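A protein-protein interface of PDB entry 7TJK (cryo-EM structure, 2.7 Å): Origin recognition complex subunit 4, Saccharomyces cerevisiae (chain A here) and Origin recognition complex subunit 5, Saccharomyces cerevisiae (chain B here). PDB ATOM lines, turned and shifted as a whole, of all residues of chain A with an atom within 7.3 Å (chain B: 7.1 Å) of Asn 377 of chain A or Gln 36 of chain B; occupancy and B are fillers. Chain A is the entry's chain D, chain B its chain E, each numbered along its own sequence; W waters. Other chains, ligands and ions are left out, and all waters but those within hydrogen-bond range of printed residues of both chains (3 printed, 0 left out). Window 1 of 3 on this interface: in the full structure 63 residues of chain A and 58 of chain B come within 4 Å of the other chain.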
ATOM      1  N   LYS A 372      21.742  20.706  -4.776  1.00  0.00           N
ATOM      2  CA  LYS A 372      22.928  19.862  -4.883  1.00  0.00           C
ATOM      3  C   LYS A 372      23.807  19.979  -3.644  1.00  0.00           C
ATOM      4  O   LYS A 372      24.362  18.978  -3.177  1.00  0.00           O
ATOM      5  CB  LYS A 372      23.719  20.229  -6.138  1.00  0.00           C
ATOM      6  CG  LYS A 372      24.904  19.320  -6.413  1.00  0.00           C
ATOM      7  CD  LYS A 372      25.595  19.681  -7.712  1.00  0.00           C
ATOM      8  CE  LYS A 372      26.876  18.889  -7.883  1.00  0.00           C
ATOM      9  NZ  LYS A 372      26.610  17.432  -8.034  1.00  0.00           N
ATOM     10  N   ASN A 373      23.947  21.190  -3.098  1.00  0.00           N
ATOM     11  CA  ASN A 373      24.799  21.370  -1.927  1.00  0.00           C
ATOM     12  C   ASN A 373      24.157  20.795  -0.669  1.00  0.00           C
ATOM     13  O   ASN A 373      24.863  20.340   0.237  1.00  0.00           O
ATOM     14  CB  ASN A 373      25.130  22.846  -1.728  1.00  0.00           C
ATOM     15  CG  ASN A 373      26.077  23.080  -0.562  1.00  0.00           C
ATOM     16  OD1 ASN A 373      25.666  23.539   0.501  1.00  0.00           O
ATOM     17  ND2 ASN A 373      27.349  22.761  -0.759  1.00  0.00           N
ATOM     18  N   GLN A 374      22.822  20.799  -0.596  1.00  0.00           N
ATOM     19  CA  GLN A 374      22.132  20.229   0.561  1.00  0.00           C
ATOM     20  C   GLN A 374      22.280  18.714   0.653  1.00  0.00           C
ATOM     21  O   GLN A 374      22.036  18.146   1.722  1.00  0.00           O
ATOM     22  CB  GLN A 374      20.643  20.590   0.539  1.00  0.00           C
ATOM     23  CG  GLN A 374      20.316  22.036   0.886  1.00  0.00           C
ATOM     24  CD  GLN A 374      20.788  22.434   2.269  1.00  0.00           C
ATOM     25  OE1 GLN A 374      20.464  21.779   3.259  1.00  0.00           O
ATOM     26  NE2 GLN A 374      21.543  23.522   2.346  1.00  0.00           N
ATOM     27  N   LEU A 375      22.657  18.043  -0.434  1.00  0.00           N
ATOM     28  CA  LEU A 375      22.861  16.601  -0.435  1.00  0.00           C
ATOM     29  C   LEU A 375      24.325  16.211  -0.602  1.00  0.00           C
ATOM     30  O   LEU A 375      24.617  15.038  -0.852  1.00  0.00           O
ATOM     31  CB  LEU A 375      22.022  15.953  -1.538  1.00  0.00           C
ATOM     32  CG  LEU A 375      20.551  16.358  -1.592  1.00  0.00           C
ATOM     33  CD1 LEU A 375      19.982  16.118  -2.978  1.00  0.00           C
ATOM     34  CD2 LEU A 375      19.757  15.606  -0.540  1.00  0.00           C
ATOM     35  N   SER A 376      25.250  17.161  -0.470  1.00  0.00           N
ATOM     36  CA  SER A 376      26.654  16.885  -0.760  1.00  0.00           C
ATOM     37  C   SER A 376      27.329  16.056   0.327  1.00  0.00           C
ATOM     38  O   SER A 376      28.306  15.357   0.044  1.00  0.00           O
ATOM     39  CB  SER A 376      27.411  18.197  -0.970  1.00  0.00           C
ATOM     40  OG  SER A 376      27.297  19.039   0.160  1.00  0.00           O
ATOM     41  N   ASN A 377      26.831  16.107   1.559  1.00  0.00           N
ATOM     42  CA  ASN A 377      27.397  15.338   2.658  1.00  0.00           C
ATOM     43  C   ASN A 377      26.526  14.155   3.055  1.00  0.00           C
ATOM     44  O   ASN A 377      26.665  13.641   4.167  1.00  0.00           O
ATOM     45  CB  ASN A 377      27.646  16.246   3.864  1.00  0.00           C
ATOM     46  CG  ASN A 377      28.797  17.206   3.638  1.00  0.00           C
ATOM     47  OD1 ASN A 377      29.643  16.979   2.776  1.00  0.00           O
ATOM     48  ND2 ASN A 377      28.830  18.286   4.403  1.00  0.00           N
ATOM     49  N   ASN A 378      25.638  13.710   2.168  1.00  0.00           N
ATOM     50  CA  ASN A 378      24.880  12.488   2.383  1.00  0.00           C
ATOM     51  C   ASN A 378      25.737  11.270   2.035  1.00  0.00           C
ATOM     52  O   ASN A 378      26.943  11.374   1.801  1.00  0.00           O
ATOM     53  CB  ASN A 378      23.599  12.504   1.552  1.00  0.00           C
ATOM     54  CG  ASN A 378      22.455  13.198   2.261  1.00  0.00           C
ATOM     55  OD1 ASN A 378      22.632  13.772   3.334  1.00  0.00           O
ATOM     56  ND2 ASN A 378      21.272  13.156   1.659  1.00  0.00           N
ATOM     57  N   LEU A 379      25.093  10.097   2.007  1.00  0.00           N
ATOM     58  CA  LEU A 379      25.809   8.848   1.746  1.00  0.00           C
ATOM     59  C   LEU A 379      26.377   8.792   0.331  1.00  0.00           C
ATOM     60  O   LEU A 379      27.493   8.301   0.124  1.00  0.00           O
ATOM     61  CB  LEU A 379      24.887   7.654   1.993  1.00  0.00           C
ATOM     62  CG  LEU A 379      24.777   7.170   3.437  1.00  0.00           C
ATOM     63  CD1 LEU A 379      23.684   6.126   3.567  1.00  0.00           C
ATOM     64  CD2 LEU A 379      26.113   6.617   3.909  1.00  0.00           C
ATOM     65  N   THR A 380      25.621   9.291  -0.652  1.00  0.00           N
ATOM     66  CA  THR A 380      26.080   9.291  -2.039  1.00  0.00           C
ATOM     67  C   THR A 380      27.282  10.213  -2.228  1.00  0.00           C
ATOM     68  O   THR A 380      28.293   9.823  -2.827  1.00  0.00           O
ATOM     69  CB  THR A 380      24.931   9.711  -2.959  1.00  0.00           C
ATOM     70  OG1 THR A 380      23.786   8.890  -2.704  1.00  0.00           O
ATOM     71  CG2 THR A 380      25.329   9.578  -4.421  1.00  0.00           C
ATOM     72  N   GLY A 381      27.193  11.436  -1.698  1.00  0.00           N
ATOM     73  CA  GLY A 381      28.294  12.374  -1.814  1.00  0.00           C
ATOM     74  C   GLY A 381      29.517  11.972  -1.018  1.00  0.00           C
ATOM     75  O   GLY A 381      30.645  12.272  -1.416  1.00  0.00           O
ATOM     76  N   ARG A 382      29.317  11.295   0.113  1.00  0.00           N
ATOM     77  CA  ARG A 382      30.448  10.786   0.877  1.00  0.00           C
ATOM     78  C   ARG A 382      31.093   9.590   0.192  1.00  0.00           C
ATOM     79  O   ARG A 382      32.311   9.408   0.298  1.00  0.00           O
ATOM     80  CB  ARG A 382      30.002  10.415   2.289  1.00  0.00           C
ATOM     81  CG  ARG A 382      30.373  11.440   3.339  1.00  0.00           C
ATOM     82  CD  ARG A 382      29.904  11.005   4.707  1.00  0.00           C
ATOM     83  NE  ARG A 382      28.479  11.253   4.878  1.00  0.00           N
ATOM     84  CZ  ARG A 382      27.631  10.404   5.439  1.00  0.00           C
ATOM     85  NH1 ARG A 382      28.035   9.236   5.910  1.00  0.00           N
ATOM     86  NH2 ARG A 382      26.347  10.733   5.527  1.00  0.00           N
ATOM     87  N   LEU A 469      33.909   8.608   8.985  1.00  0.00           N
ATOM     88  CA  LEU A 469      32.965   9.116   7.997  1.00  0.00           C
ATOM     89  C   LEU A 469      31.579   8.484   8.101  1.00  0.00           C
ATOM     90  O   LEU A 469      30.771   8.665   7.183  1.00  0.00           O
ATOM     91  CB  LEU A 469      33.516   8.906   6.586  1.00  0.00           C
ATOM     92  CG  LEU A 469      34.568   9.909   6.116  1.00  0.00           C
ATOM     93  CD1 LEU A 469      35.224   9.427   4.836  1.00  0.00           C
ATOM     94  CD2 LEU A 469      33.953  11.282   5.926  1.00  0.00           C
ATOM     95  N   GLN B  14      30.200  28.450  -0.854  1.00  0.00           N
ATOM     96  CA  GLN B  14      30.130  28.627   0.592  1.00  0.00           C
ATOM     97  C   GLN B  14      30.378  30.078   0.983  1.00  0.00           C
ATOM     98  O   GLN B  14      29.697  30.610   1.864  1.00  0.00           O
ATOM     99  CB  GLN B  14      31.137  27.703   1.276  1.00  0.00           C
ATOM    100  CG  GLN B  14      30.718  26.244   1.321  1.00  0.00           C
ATOM    101  CD  GLN B  14      31.017  25.499   0.037  1.00  0.00           C
ATOM    102  OE1 GLN B  14      31.609  26.045  -0.891  1.00  0.00           O
ATOM    103  NE2 GLN B  14      30.603  24.244  -0.022  1.00  0.00           N
ATOM    104  N   ILE B  34      24.094  27.196  10.305  1.00  0.00           N
ATOM    105  CA  ILE B  34      24.896  25.994  10.510  1.00  0.00           C
ATOM    106  C   ILE B  34      25.857  25.847   9.338  1.00  0.00           C
ATOM    107  O   ILE B  34      25.455  26.014   8.183  1.00  0.00           O
ATOM    108  CB  ILE B  34      24.004  24.746  10.665  1.00  0.00           C
ATOM    109  CG1 ILE B  34      23.102  24.887  11.893  1.00  0.00           C
ATOM    110  CG2 ILE B  34      24.838  23.479  10.786  1.00  0.00           C
ATOM    111  CD1 ILE B  34      22.087  23.782  12.039  1.00  0.00           C
ATOM    112  N   LEU B  35      27.131  25.590   9.638  1.00  0.00           N
ATOM    113  CA  LEU B  35      28.125  25.192   8.642  1.00  0.00           C
ATOM    114  C   LEU B  35      28.506  23.745   8.918  1.00  0.00           C
ATOM    115  O   LEU B  35      29.238  23.463   9.870  1.00  0.00           O
ATOM    116  CB  LEU B  35      29.361  26.090   8.680  1.00  0.00           C
ATOM    117  CG  LEU B  35      29.247  27.612   8.626  1.00  0.00           C
ATOM    118  CD1 LEU B  35      30.609  28.202   8.302  1.00  0.00           C
ATOM    119  CD2 LEU B  35      28.223  28.042   7.598  1.00  0.00           C
ATOM    120  N   GLN B  36      28.030  22.830   8.082  1.00  0.00           N
ATOM    121  CA  GLN B  36      28.225  21.403   8.305  1.00  0.00           C
ATOM    122  C   GLN B  36      29.237  20.853   7.312  1.00  0.00           C
ATOM    123  O   GLN B  36      29.116  21.080   6.108  1.00  0.00           O
ATOM    124  CB  GLN B  36      26.901  20.643   8.188  1.00  0.00           C
ATOM    125  CG  GLN B  36      26.977  19.181   8.615  1.00  0.00           C
ATOM    126  CD  GLN B  36      27.230  18.236   7.452  1.00  0.00           C
ATOM    127  OE1 GLN B  36      26.735  18.450   6.348  1.00  0.00           O
ATOM    128  NE2 GLN B  36      28.018  17.197   7.694  1.00  0.00           N
ATOM    129  N   GLY B  37      30.213  20.117   7.820  1.00  0.00           N
ATOM    130  CA  GLY B  37      31.191  19.475   6.966  1.00  0.00           C
ATOM    131  C   GLY B  37      32.128  18.642   7.811  1.00  0.00           C
ATOM    132  O   GLY B  37      32.291  18.875   9.011  1.00  0.00           O
ATOM    133  N   TYR B  38      32.746  17.664   7.160  1.00  0.00           N
ATOM    134  CA  TYR B  38      33.660  16.785   7.872  1.00  0.00           C
ATOM    135  C   TYR B  38      35.020  17.461   8.042  1.00  0.00           C
ATOM    136  O   TYR B  38      35.230  18.608   7.637  1.00  0.00           O
ATOM    137  CB  TYR B  38      33.757  15.438   7.163  1.00  0.00           C
ATOM    138  CG  TYR B  38      32.554  14.567   7.446  1.00  0.00           C
ATOM    139  CD1 TYR B  38      32.539  13.706   8.533  1.00  0.00           C
ATOM    140  CD2 TYR B  38      31.419  14.634   6.645  1.00  0.00           C
ATOM    141  CE1 TYR B  38      31.437  12.920   8.807  1.00  0.00           C
ATOM    142  CE2 TYR B  38      30.310  13.855   6.911  1.00  0.00           C
ATOM    143  CZ  TYR B  38      30.327  12.999   7.992  1.00  0.00           C
ATOM    144  OH  TYR B  38      29.229  12.218   8.262  1.00  0.00           O
ATOM    145  N   THR B  41      37.660  20.269   5.735  1.00  0.00           N
ATOM    146  CA  THR B  41      36.905  20.730   4.579  1.00  0.00           C
ATOM    147  C   THR B  41      36.880  22.246   4.452  1.00  0.00           C
ATOM    148  O   THR B  41      36.111  22.772   3.644  1.00  0.00           O
ATOM    149  CB  THR B  41      35.474  20.191   4.630  1.00  0.00           C
ATOM    150  OG1 THR B  41      34.917  20.416   5.931  1.00  0.00           O
ATOM    151  CG2 THR B  41      35.463  18.703   4.327  1.00  0.00           C
ATOM    152  N   LYS B  43      35.994  24.698   6.654  1.00  0.00           N
ATOM    153  CA  LYS B  43      34.934  25.464   7.307  1.00  0.00           C
ATOM    154  C   LYS B  43      35.506  26.633   8.101  1.00  0.00           C
ATOM    155  O   LYS B  43      35.091  27.790   7.925  1.00  0.00           O
ATOM    156  CB  LYS B  43      34.131  24.544   8.227  1.00  0.00           C
ATOM    157  CG  LYS B  43      33.507  23.355   7.528  1.00  0.00           C
ATOM    158  CD  LYS B  43      32.674  22.536   8.489  1.00  0.00           C
ATOM    159  CE  LYS B  43      33.555  21.853   9.529  1.00  0.00           C
ATOM    160  NZ  LYS B  43      34.646  21.034   8.944  1.00  0.00           N
ATOM    161  N   TYR B 168      26.777  27.979  14.000  1.00  0.00           N
ATOM    162  CA  TYR B 168      27.213  26.671  14.459  1.00  0.00           C
ATOM    163  C   TYR B 168      28.043  25.972  13.393  1.00  0.00           C
ATOM    164  O   TYR B 168      27.829  26.149  12.192  1.00  0.00           O
ATOM    165  CB  TYR B 168      26.023  25.788  14.834  1.00  0.00           C
ATOM    166  CG  TYR B 168      25.044  26.428  15.782  1.00  0.00           C
ATOM    167  CD1 TYR B 168      25.242  26.372  17.156  1.00  0.00           C
ATOM    168  CD2 TYR B 168      23.910  27.076  15.304  1.00  0.00           C
ATOM    169  CE1 TYR B 168      24.345  26.954  18.026  1.00  0.00           C
ATOM    170  CE2 TYR B 168      23.011  27.657  16.163  1.00  0.00           C
ATOM    171  CZ  TYR B 168      23.228  27.589  17.522  1.00  0.00           C
ATOM    172  OH  TYR B 168      22.326  28.174  18.374  1.00  0.00           O
ATOM    173  N   THR B 169      29.003  25.180  13.853  1.00  0.00           N
ATOM    174  CA  THR B 169      29.821  24.340  12.996  1.00  0.00           C
ATOM    175  C   THR B 169      29.651  22.893  13.436  1.00  0.00           C
ATOM    176  O   THR B 169      29.801  22.583  14.620  1.00  0.00           O
ATOM    177  CB  THR B 169      31.291  24.767  13.055  1.00  0.00           C
ATOM    178  OG1 THR B 169      31.416  26.125  12.614  1.00  0.00           O
ATOM    179  CG2 THR B 169      32.136  23.891  12.190  1.00  0.00           C
ATOM    180  N   MET B 170      29.330  22.017  12.487  1.00  0.00           N
ATOM    181  CA  MET B 170      29.051  20.617  12.776  1.00  0.00           C
ATOM    182  C   MET B 170      29.923  19.718  11.915  1.00  0.00           C
ATOM    183  O   MET B 170      30.354  20.103  10.826  1.00  0.00           O
ATOM    184  CB  MET B 170      27.579  20.275  12.536  1.00  0.00           C
ATOM    185  CG  MET B 170      26.622  20.942  13.494  1.00  0.00           C
ATOM    186  SD  MET B 170      24.915  20.502  13.148  1.00  0.00           S
ATOM    187  CE  MET B 170      24.072  21.506  14.360  1.00  0.00           C
ATOM    188  N   LEU B 171      30.170  18.507  12.413  1.00  0.00           N
ATOM    189  CA  LEU B 171      30.954  17.508  11.695  1.00  0.00           C
ATOM    190  C   LEU B 171      30.081  16.418  11.084  1.00  0.00           C
ATOM    191  O   LEU B 171      30.199  16.120   9.892  1.00  0.00           O
ATOM    192  CB  LEU B 171      32.006  16.886  12.625  1.00  0.00           C
ATOM    193  CG  LEU B 171      33.315  17.658  12.803  1.00  0.00           C
ATOM    194  CD1 LEU B 171      34.094  17.134  13.998  1.00  0.00           C
ATOM    195  CD2 LEU B 171      34.155  17.586  11.548  1.00  0.00           C
ATOM    196  N   GLU B 172      29.200  15.819  11.878  1.00  0.00           N
ATOM    197  CA  GLU B 172      28.481  14.622  11.470  1.00  0.00           C
ATOM    198  C   GLU B 172      27.170  14.980  10.780  1.00  0.00           C
ATOM    199  O   GLU B 172      26.480  15.921  11.177  1.00  0.00           O
ATOM    200  CB  GLU B 172      28.206  13.727  12.678  1.00  0.00           C
ATOM    201  CG  GLU B 172      29.450  13.138  13.323  1.00  0.00           C
ATOM    202  CD  GLU B 172      30.177  12.145  12.433  1.00  0.00           C
ATOM    203  OE1 GLU B 172      29.514  11.451  11.633  1.00  0.00           O
ATOM    204  OE2 GLU B 172      31.418  12.052  12.539  1.00  0.00           O
ATOM    205  N   THR B 173      26.838  14.215   9.737  1.00  0.00           N
ATOM    206  CA  THR B 173      25.594  14.434   9.006  1.00  0.00           C
ATOM    207  C   THR B 173      24.376  14.010   9.822  1.00  0.00           C
ATOM    208  O   THR B 173      23.332  14.668   9.758  1.00  0.00           O
ATOM    209  CB  THR B 173      25.647  13.684   7.671  1.00  0.00           C
ATOM    210  OG1 THR B 173      26.868  14.002   6.994  1.00  0.00           O
ATOM    211  CG2 THR B 173      24.489  14.070   6.771  1.00  0.00           C
ATOM    212  N   SER B 174      24.498  12.934  10.608  1.00  0.00           N
ATOM    213  CA  SER B 174      23.355  12.406  11.350  1.00  0.00           C
ATOM    214  C   SER B 174      22.936  13.336  12.485  1.00  0.00           C
ATOM    215  O   SER B 174      21.737  13.474  12.772  1.00  0.00           O
ATOM    216  CB  SER B 174      23.687  11.015  11.891  1.00  0.00           C
ATOM    217  OG  SER B 174      24.662  11.083  12.914  1.00  0.00           O
ATOM    218  N   LEU B 176      23.225  16.623  12.404  1.00  0.00           N
ATOM    219  CA  LEU B 176      22.501  17.703  11.741  1.00  0.00           C
ATOM    220  C   LEU B 176      21.110  17.258  11.308  1.00  0.00           C
ATOM    221  O   LEU B 176      20.137  18.010  11.445  1.00  0.00           O
ATOM    222  CB  LEU B 176      23.304  18.199  10.542  1.00  0.00           C
ATOM    223  CG  LEU B 176      22.610  19.166   9.583  1.00  0.00           C
ATOM    224  CD1 LEU B 176      22.591  20.568  10.149  1.00  0.00           C
ATOM    225  CD2 LEU B 176      23.287  19.142   8.236  1.00  0.00           C
ATOM    226  N   GLN B 177      20.993  16.032  10.805  1.00  0.00           N
ATOM    227  CA  GLN B 177      19.720  15.518  10.323  1.00  0.00           C
ATOM    228  C   GLN B 177      18.755  15.175  11.451  1.00  0.00           C
ATOM    229  O   GLN B 177      17.568  14.966  11.185  1.00  0.00           O
ATOM    230  CB  GLN B 177      19.982  14.310   9.424  1.00  0.00           C
ATOM    231  CG  GLN B 177      20.497  14.722   8.046  1.00  0.00           C
ATOM    232  CD  GLN B 177      20.916  13.553   7.181  1.00  0.00           C
ATOM    233  OE1 GLN B 177      20.921  12.409   7.627  1.00  0.00           O
ATOM    234  NE2 GLN B 177      21.266  13.837   5.931  1.00  0.00           N
ATOM    235  N   THR B 186      21.509  26.051   6.466  1.00  0.00           N
ATOM    236  CA  THR B 186      22.721  25.256   6.566  1.00  0.00           C
ATOM    237  C   THR B 186      23.521  25.400   5.282  1.00  0.00           C
ATOM    238  O   THR B 186      22.980  25.248   4.184  1.00  0.00           O
ATOM    239  CB  THR B 186      22.399  23.775   6.824  1.00  0.00           C
ATOM    240  OG1 THR B 186      21.469  23.667   7.908  1.00  0.00           O
ATOM    241  CG2 THR B 186      23.659  23.001   7.172  1.00  0.00           C
ATOM    242  N   VAL B 187      24.805  25.702   5.430  1.00  0.00           N
ATOM    243  CA  VAL B 187      25.775  25.670   4.345  1.00  0.00           C
ATOM    244  C   VAL B 187      26.636  24.436   4.552  1.00  0.00           C
ATOM    245  O   VAL B 187      27.159  24.213   5.652  1.00  0.00           O
ATOM    246  CB  VAL B 187      26.630  26.947   4.313  1.00  0.00           C
ATOM    247  CG1 VAL B 187      27.469  26.995   3.046  1.00  0.00           C
ATOM    248  CG2 VAL B 187      25.747  28.176   4.431  1.00  0.00           C
ATOM    249  N   MET B 188      26.777  23.635   3.509  1.00  0.00           N
ATOM    250  CA  MET B 188      27.498  22.378   3.617  1.00  0.00           C
ATOM    251  C   MET B 188      28.821  22.471   2.876  1.00  0.00           C
ATOM    252  O   MET B 188      28.916  23.095   1.817  1.00  0.00           O
ATOM    253  CB  MET B 188      26.657  21.216   3.086  1.00  0.00           C
ATOM    254  CG  MET B 188      25.440  20.952   3.955  1.00  0.00           C
ATOM    255  SD  MET B 188      24.413  19.602   3.379  1.00  0.00           S
ATOM    256  CE  MET B 188      23.072  19.666   4.563  1.00  0.00           C
ATOM    257  N   PHE B 189      29.844  21.854   3.461  1.00  0.00           N
ATOM    258  CA  PHE B 189      31.217  21.890   2.964  1.00  0.00           C
ATOM    259  C   PHE B 189      31.564  20.463   2.567  1.00  0.00           C
ATOM    260  O   PHE B 189      31.939  19.648   3.425  1.00  0.00           O
ATOM    261  CB  PHE B 189      32.181  22.416   4.028  1.00  0.00           C
ATOM    262  CG  PHE B 189      32.098  23.902   4.264  1.00  0.00           C
ATOM    263  CD1 PHE B 189      31.010  24.466   4.917  1.00  0.00           C
ATOM    264  CD2 PHE B 189      33.131  24.731   3.859  1.00  0.00           C
ATOM    265  CE1 PHE B 189      30.941  25.827   5.137  1.00  0.00           C
ATOM    266  CE2 PHE B 189      33.070  26.095   4.082  1.00  0.00           C
ATOM    267  CZ  PHE B 189      31.973  26.641   4.721  1.00  0.00           C
ATOM    268  N   PRO B 190      31.425  20.104   1.293  1.00  0.00           N
ATOM    269  CA  PRO B 190      31.802  18.755   0.862  1.00  0.00           C
ATOM    270  C   PRO B 190      33.310  18.567   0.881  1.00  0.00           C
ATOM    271  O   PRO B 190      34.087  19.523   0.848  1.00  0.00           O
ATOM    272  CB  PRO B 190      31.248  18.665  -0.562  1.00  0.00           C
ATOM    273  CG  PRO B 190      31.142  20.073  -1.011  1.00  0.00           C
ATOM    274  CD  PRO B 190      30.810  20.876   0.202  1.00  0.00           C
ATOM    275  N   ARG B 191      33.713  17.302   0.964  1.00  0.00           N
ATOM    276  CA  ARG B 191      35.125  16.954   0.987  1.00  0.00           C
ATOM    277  C   ARG B 191      35.778  17.258  -0.355  1.00  0.00           C
ATOM    278  O   ARG B 191      35.179  17.082  -1.418  1.00  0.00           O
ATOM    279  CB  ARG B 191      35.302  15.478   1.337  1.00  0.00           C
ATOM    280  CG  ARG B 191      34.705  15.091   2.676  1.00  0.00           C
ATOM    281  CD  ARG B 191      34.946  13.630   2.989  1.00  0.00           C
ATOM    282  NE  ARG B 191      36.333  13.371   3.353  1.00  0.00           N
ATOM    283  CZ  ARG B 191      37.015  12.293   2.993  1.00  0.00           C
ATOM    284  NH1 ARG B 191      36.469  11.349   2.245  1.00  0.00           N
ATOM    285  NH2 ARG B 191      38.276  12.159   3.392  1.00  0.00           N
HETATM  286  O   HOH W   1      32.359  17.454   4.537  1.00  0.00           O
HETATM  287  O   HOH W   2      24.314  16.899   2.998  1.00  0.00           O
HETATM  288  O   HOH W   3      19.471  24.427   5.102  1.00  0.00           O
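Of the 12 printed residues of chain A, 7 touch a printed residue of chain B.
Gln 14 of chain B touches Asn 373 of chain A (NE2 to ND2, 3.7 Å). Met 188 of chain B touches Ser 376 of chain A (CB to OG, 3.7 Å). Asn 377 of chain A touches Gly 37 of chain B (ND2 to CA, 3.7 Å). CB of Met 188 of chain B touches ND2 of Asn 377 of chain A (3.9 Å). Asn 377 of chain A touches Phe 189 of chain B. Pro 190 of chain B touches Asn 377 of chain A (CA to OD1, 3.4 Å). Asn 378 of chain A touches Thr 173 of chain B (OD1 to CG2, 3.9 Å). Arg 382 of chain A touches Tyr 38 of chain B (NE to OH, 3.6 Å). CD2 of Leu 469 of chain A touches CD1 of Tyr 38 of chain B, 3.8 Å away. Leu 469 of chain A touches Arg 191 of chain B.
Of chain B, only Gln 36 (2.9 Å), Gly 37 (3.7 Å), Thr 173 (2.9 Å), Met 188 (3.9 Å), Phe 189 (3.5 Å) and Pro 190 (3.4 Å) come within 4 Å of Asn 377 of chain A. Gln 36 of chain B touches just one residue of chain A: Asn 377. Printed residues of chain A within 4 Å of Thr 173 of chain B: Asn 377, Asn 378 and Arg 382. Printed residues of chain A within 4 Å of Phe 189 of chain B: Asn 377 (3.5 Å). The nearest residue of chain A that does not touch Gln 36 of chain B is Ser 376 of chain A (6.2 Å). The nearest printed residue of chain B that does not touch Leu 469 of chain A is Glu 172 of chain B (5.1 Å).
Water W1 lies within hydrogen-bond range of O of Phe 189 of chain B, N of Tyr 38 of chain B and OD1 of Asn 377 of chain A. Water W2 lies within hydrogen-bond range of the side-chain sulfur of Met 188 of chain B, the backbone carbonyl oxygen of Gln 374 of chain A and the backbone NH of Asn 377 of chain A. Water W3 lies within hydrogen-bond range of N of Thr 186 of chain B and OE1 of Gln 374 of chain A.
The backbone carbonyl oxygen (O) of Asn 377 of chain A lies within hydrogen-bond range of the guanidinium group (NE) of Arg 382 of chain A. The guanidinium group of Arg 382 of chain A sits close to the backbone carbonyl oxygen of Asn 378 of chain A (3.4 Å). NE2 of Gln 14 of chain B is in hydrogen-bond range of O of Met 188 of chain B. The backbone carbonyl oxygen (O) of Gln 36 of chain B sits at hydrogen-bond distance from the backbone NH (N) of Phe 189 of chain B (2.9 Å). The backbone carbonyl oxygen of Gly 37 of chain B is in hydrogen-bond range of the side-chain amino group of Lys 43 of chain B (3.2 Å). The backbone carbonyl oxygen of Tyr 38 of chain B sits at hydrogen-bond distance from the side-chain amino group of Lys 43 of chain B (2.8 Å).
The side-chain amide nitrogen of Asn 373 of chain A is in hydrogen-bond range of the backbone carbonyl oxygen of Met 188 of chain B, 3.0 Å away. The side-chain amide nitrogen (NE2) of Gln 374 of chain A lies within hydrogen-bond range of the backbone carbonyl oxygen (O) of Thr 186 of chain B (2.9 Å). The side-chain amide oxygen (OE1) of Gln 36 of chain B sits at hydrogen-bond distance from the side-chain amide nitrogen (ND2) of Asn 377 of chain A (2.9 Å). The backbone carbonyl oxygen of Asn 377 of chain A lies within hydrogen-bond range of the side-chain hydroxyl of Thr 173 of chain B (2.9 Å). The side-chain amide oxygen (OD1) of Asn 378 of chain A is in hydrogen-bond range of the side-chain amide nitrogen (NE2) of Gln 177 of chain B (2.9 Å). The backbone carbonyl oxygen (O) of Gln 374 of chain A lies close to the side-chain sulfur (SD) of Met 188 of chain B, at 3.2 Å.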
